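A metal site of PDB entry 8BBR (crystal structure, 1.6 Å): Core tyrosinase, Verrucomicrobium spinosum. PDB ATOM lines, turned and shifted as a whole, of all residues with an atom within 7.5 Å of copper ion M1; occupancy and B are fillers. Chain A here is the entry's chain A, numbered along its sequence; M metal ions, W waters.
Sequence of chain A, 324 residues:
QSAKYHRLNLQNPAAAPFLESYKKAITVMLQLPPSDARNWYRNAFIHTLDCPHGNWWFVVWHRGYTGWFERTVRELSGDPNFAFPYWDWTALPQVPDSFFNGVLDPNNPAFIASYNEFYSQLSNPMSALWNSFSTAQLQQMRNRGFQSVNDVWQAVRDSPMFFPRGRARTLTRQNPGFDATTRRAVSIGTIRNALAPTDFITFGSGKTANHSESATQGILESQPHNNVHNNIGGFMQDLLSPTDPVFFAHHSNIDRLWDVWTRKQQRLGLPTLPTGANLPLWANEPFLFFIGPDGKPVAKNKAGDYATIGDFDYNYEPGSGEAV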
ATOM      1  N   HIS A  47     -17.760   3.752 -26.658  1.00  0.00           N
ATOM      2  CA  HIS A  47     -19.241   3.869 -26.627  1.00  0.00           C
ATOM      3  C   HIS A  47     -19.658   4.871 -25.536  1.00  0.00           C
ATOM      4  O   HIS A  47     -20.425   5.807 -25.840  1.00  0.00           O
ATOM      5  CB  HIS A  47     -19.836   2.474 -26.464  1.00  0.00           C
ATOM      6  CG  HIS A  47     -21.332   2.446 -26.518  1.00  0.00           C
ATOM      7  ND1 HIS A  47     -22.098   2.597 -25.412  1.00  0.00           N
ATOM      8  CD2 HIS A  47     -22.178   2.230 -27.551  1.00  0.00           C
ATOM      9  CE1 HIS A  47     -23.382   2.494 -25.745  1.00  0.00           C
ATOM     10  NE2 HIS A  47     -23.446   2.270 -27.062  1.00  0.00           N
ATOM     11  N   HIS A  53     -27.189   8.751 -28.597  1.00  0.00           N
ATOM     12  CA  HIS A  53     -28.499   8.069 -28.459  1.00  0.00           C
ATOM     13  C   HIS A  53     -29.589   9.163 -28.497  1.00  0.00           C
ATOM     14  O   HIS A  53     -29.376  10.304 -28.066  1.00  0.00           O
ATOM     15  CB  HIS A  53     -28.400   6.994 -27.352  1.00  0.00           C
ATOM     16  CG  HIS A  53     -27.205   6.074 -27.459  1.00  0.00           C
ATOM     17  ND1 HIS A  53     -25.951   6.456 -26.988  1.00  0.00           N
ATOM     18  CD2 HIS A  53     -27.035   4.822 -27.989  1.00  0.00           C
ATOM     19  CE1 HIS A  53     -25.054   5.496 -27.208  1.00  0.00           C
ATOM     20  NE2 HIS A  53     -25.704   4.444 -27.832  1.00  0.00           N
ATOM     21  N   PHE A  58     -27.667   8.108 -34.700  1.00  0.00           N
ATOM     22  CA  PHE A  58     -27.840   6.737 -34.150  1.00  0.00           C
ATOM     23  C   PHE A  58     -27.310   5.640 -35.117  1.00  0.00           C
ATOM     24  O   PHE A  58     -26.322   4.940 -34.754  1.00  0.00           O
ATOM     25  CB  PHE A  58     -29.311   6.525 -33.812  1.00  0.00           C
ATOM     26  CG  PHE A  58     -29.680   5.109 -33.517  1.00  0.00           C
ATOM     27  CD1 PHE A  58     -29.048   4.428 -32.486  1.00  0.00           C
ATOM     28  CD2 PHE A  58     -30.611   4.446 -34.296  1.00  0.00           C
ATOM     29  CE1 PHE A  58     -29.365   3.100 -32.228  1.00  0.00           C
ATOM     30  CE2 PHE A  58     -30.934   3.122 -34.032  1.00  0.00           C
ATOM     31  CZ  PHE A  58     -30.300   2.459 -33.009  1.00  0.00           C
ATOM     32  N   HIS A  62     -23.242   3.913 -35.103  1.00  0.00           N
ATOM     33  CA  HIS A  62     -23.201   2.455 -34.811  1.00  0.00           C
ATOM     34  C   HIS A  62     -22.621   1.647 -35.996  1.00  0.00           C
ATOM     35  O   HIS A  62     -21.906   0.696 -35.756  1.00  0.00           O
ATOM     36  CB  HIS A  62     -24.556   1.975 -34.271  1.00  0.00           C
ATOM     37  CG  HIS A  62     -24.767   2.406 -32.849  1.00  0.00           C
ATOM     38  ND1 HIS A  62     -25.402   3.597 -32.503  1.00  0.00           N
ATOM     39  CD2 HIS A  62     -24.469   1.792 -31.664  1.00  0.00           C
ATOM     40  CE1 HIS A  62     -25.433   3.714 -31.172  1.00  0.00           C
ATOM     41  NE2 HIS A  62     -24.885   2.597 -30.627  1.00  0.00           N
ATOM     42  N   HIS A 225     -34.525  -1.493 -30.747  1.00  0.00           N
ATOM     43  CA  HIS A 225     -33.169  -1.217 -30.241  1.00  0.00           C
ATOM     44  C   HIS A 225     -33.167  -1.006 -28.722  1.00  0.00           C
ATOM     45  O   HIS A 225     -32.426  -1.754 -28.019  1.00  0.00           O
ATOM     46  CB  HIS A 225     -32.523  -0.050 -30.987  1.00  0.00           C
ATOM     47  CG  HIS A 225     -31.239   0.318 -30.339  1.00  0.00           C
ATOM     48  ND1 HIS A 225     -31.116   1.363 -29.435  1.00  0.00           N
ATOM     49  CD2 HIS A 225     -29.996  -0.239 -30.436  1.00  0.00           C
ATOM     50  CE1 HIS A 225     -29.865   1.431 -29.023  1.00  0.00           C
ATOM     51  NE2 HIS A 225     -29.164   0.456 -29.616  1.00  0.00           N
ATOM     52  N   ASN A 226     -33.947  -0.030 -28.211  1.00  0.00           N
ATOM     53  CA  ASN A 226     -33.874   0.377 -26.779  1.00  0.00           C
ATOM     54  C   ASN A 226     -34.451  -0.763 -25.947  1.00  0.00           C
ATOM     55  O   ASN A 226     -33.890  -1.029 -24.894  1.00  0.00           O
ATOM     56  CB  ASN A 226     -34.545   1.715 -26.508  1.00  0.00           C
ATOM     57  CG  ASN A 226     -33.815   2.911 -27.115  1.00  0.00           C
ATOM     58  OD1 ASN A 226     -32.689   2.786 -27.601  1.00  0.00           O
ATOM     59  ND2 ASN A 226     -34.420   4.091 -27.026  1.00  0.00           N
ATOM     60  N   HIS A 229     -32.026  -3.787 -25.476  1.00  0.00           N
ATOM     61  CA  HIS A 229     -30.964  -3.320 -24.526  1.00  0.00           C
ATOM     62  C   HIS A 229     -31.465  -3.453 -23.067  1.00  0.00           C
ATOM     63  O   HIS A 229     -30.777  -4.115 -22.230  1.00  0.00           O
ATOM     64  CB  HIS A 229     -30.584  -1.863 -24.851  1.00  0.00           C
ATOM     65  CG  HIS A 229     -29.402  -1.714 -25.756  1.00  0.00           C
ATOM     66  ND1 HIS A 229     -28.122  -1.865 -25.303  1.00  0.00           N
ATOM     67  CD2 HIS A 229     -29.296  -1.301 -27.054  1.00  0.00           C
ATOM     68  CE1 HIS A 229     -27.262  -1.611 -26.284  1.00  0.00           C
ATOM     69  NE2 HIS A 229     -27.961  -1.372 -27.395  1.00  0.00           N
ATOM     70  N   MET A 236     -25.947  -4.265 -20.819  1.00  0.00           N
ATOM     71  CA  MET A 236     -26.759  -3.872 -22.003  1.00  0.00           C
ATOM     72  C   MET A 236     -27.769  -2.767 -21.677  1.00  0.00           C
ATOM     73  O   MET A 236     -28.151  -2.061 -22.613  1.00  0.00           O
ATOM     74  CB  MET A 236     -27.430  -5.078 -22.667  1.00  0.00           C
ATOM     75  CG  MET A 236     -26.463  -5.949 -23.487  1.00  0.00           C
ATOM     76  SD  MET A 236     -25.880  -5.023 -24.949  1.00  0.00           S
ATOM     77  CE  MET A 236     -27.276  -5.213 -26.060  1.00  0.00           C
ATOM     78  N   SER A 241     -22.597  -0.948 -22.401  1.00  0.00           N
ATOM     79  CA  SER A 241     -23.273  -2.061 -23.126  1.00  0.00           C
ATOM     80  C   SER A 241     -22.307  -2.921 -23.968  1.00  0.00           C
ATOM     81  O   SER A 241     -22.502  -4.127 -24.042  1.00  0.00           O
ATOM     82  CB  SER A 241     -24.485  -1.570 -23.914  1.00  0.00           C
ATOM     83  OG  SER A 241     -24.113  -0.490 -24.769  1.00  0.00           O
ATOM     84  N   PHE A 247     -23.803  -7.349 -27.731  1.00  0.00           N
ATOM     85  CA  PHE A 247     -23.941  -5.965 -28.249  1.00  0.00           C
ATOM     86  C   PHE A 247     -23.695  -5.959 -29.760  1.00  0.00           C
ATOM     87  O   PHE A 247     -24.464  -5.309 -30.529  1.00  0.00           O
ATOM     88  CB  PHE A 247     -23.023  -4.978 -27.503  1.00  0.00           C
ATOM     89  CG  PHE A 247     -23.036  -3.581 -28.082  1.00  0.00           C
ATOM     90  CD1 PHE A 247     -22.280  -3.267 -29.187  1.00  0.00           C
ATOM     91  CD2 PHE A 247     -23.813  -2.588 -27.492  1.00  0.00           C
ATOM     92  CE1 PHE A 247     -22.312  -1.978 -29.716  1.00  0.00           C
ATOM     93  CE2 PHE A 247     -23.859  -1.296 -28.019  1.00  0.00           C
ATOM     94  CZ  PHE A 247     -23.076  -0.996 -29.123  1.00  0.00           C
ATOM     95  N   HIS A 250     -26.451  -7.695 -31.756  1.00  0.00           N
ATOM     96  CA  HIS A 250     -27.623  -6.781 -31.698  1.00  0.00           C
ATOM     97  C   HIS A 250     -27.407  -5.717 -32.790  1.00  0.00           C
ATOM     98  O   HIS A 250     -28.275  -5.515 -33.589  1.00  0.00           O
ATOM     99  CB  HIS A 250     -27.767  -6.175 -30.296  1.00  0.00           C
ATOM    100  CG  HIS A 250     -28.898  -5.216 -30.100  1.00  0.00           C
ATOM    101  ND1 HIS A 250     -30.163  -5.431 -30.580  1.00  0.00           N
ATOM    102  CD2 HIS A 250     -28.972  -4.076 -29.377  1.00  0.00           C
ATOM    103  CE1 HIS A 250     -30.958  -4.468 -30.204  1.00  0.00           C
ATOM    104  NE2 HIS A 250     -30.255  -3.606 -29.478  1.00  0.00           N
ATOM    105  N   HIS A 251     -26.217  -5.130 -32.827  1.00  0.00           N
ATOM    106  CA  HIS A 251     -25.914  -3.987 -33.749  1.00  0.00           C
ATOM    107  C   HIS A 251     -25.697  -4.457 -35.201  1.00  0.00           C
ATOM    108  O   HIS A 251     -25.971  -3.657 -36.131  1.00  0.00           O
ATOM    109  CB  HIS A 251     -24.814  -3.116 -33.169  1.00  0.00           C
ATOM    110  CG  HIS A 251     -25.444  -2.083 -32.321  1.00  0.00           C
ATOM    111  ND1 HIS A 251     -26.110  -0.988 -32.866  1.00  0.00           N
ATOM    112  CD2 HIS A 251     -25.732  -2.093 -31.000  1.00  0.00           C
ATOM    113  CE1 HIS A 251     -26.706  -0.333 -31.890  1.00  0.00           C
ATOM    114  NE2 HIS A 251     -26.477  -0.996 -30.749  1.00  0.00           N
ATOM    115  N   ILE A 254     -29.289  -4.368 -36.277  1.00  0.00           N
ATOM    116  CA  ILE A 254     -29.767  -2.973 -36.470  1.00  0.00           C
ATOM    117  C   ILE A 254     -29.220  -2.504 -37.817  1.00  0.00           C
ATOM    118  O   ILE A 254     -29.986  -1.908 -38.623  1.00  0.00           O
ATOM    119  CB  ILE A 254     -29.345  -2.086 -35.291  1.00  0.00           C
ATOM    120  CG1 ILE A 254     -30.164  -2.390 -34.027  1.00  0.00           C
ATOM    121  CG2 ILE A 254     -29.406  -0.613 -35.667  1.00  0.00           C
ATOM    122  CD1 ILE A 254     -31.641  -2.143 -34.158  1.00  0.00           C
HETATM  123 CU    CU M   1     -27.329  -0.376 -28.974  1.00  0.00          CU
HETATM  124 CU    CU M   2     -24.981   2.494 -28.468  1.00  0.00          CU
HETATM  125  O   HOH W   1     -26.832   1.786 -27.807  1.00  0.00           O
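ND1 of His 229 lies within hydrogen-bond range of O of Met 236 (2.7 Å).
O of His 225 is in hydrogen-bond range of NE2 of His 250 (3.2 Å).
A ring nitrogen (ND1) of His 225 lies within hydrogen-bond range of the side-chain amide oxygen (OD1) of Asn 226 (2.8 Å).
Phe 247 touches copper ion M1 (CE2 to CU, 3.7 Å).
Four residues have an atom within 4 Å of copper ion M1: His 225, His 229, Phe 247 and His 251.
The nearest printed residue that does not touch copper ion M1 is His 250 (4.1 Å).
Copper ion M1 is bound by a ring nitrogen (NE2) of His 229 (2.0 Å), a ring nitrogen (NE2) of His 251 (2.1 Å), a ring nitrogen (NE2) of His 225 (2.1 Å) and water W1 (2.5 Å).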
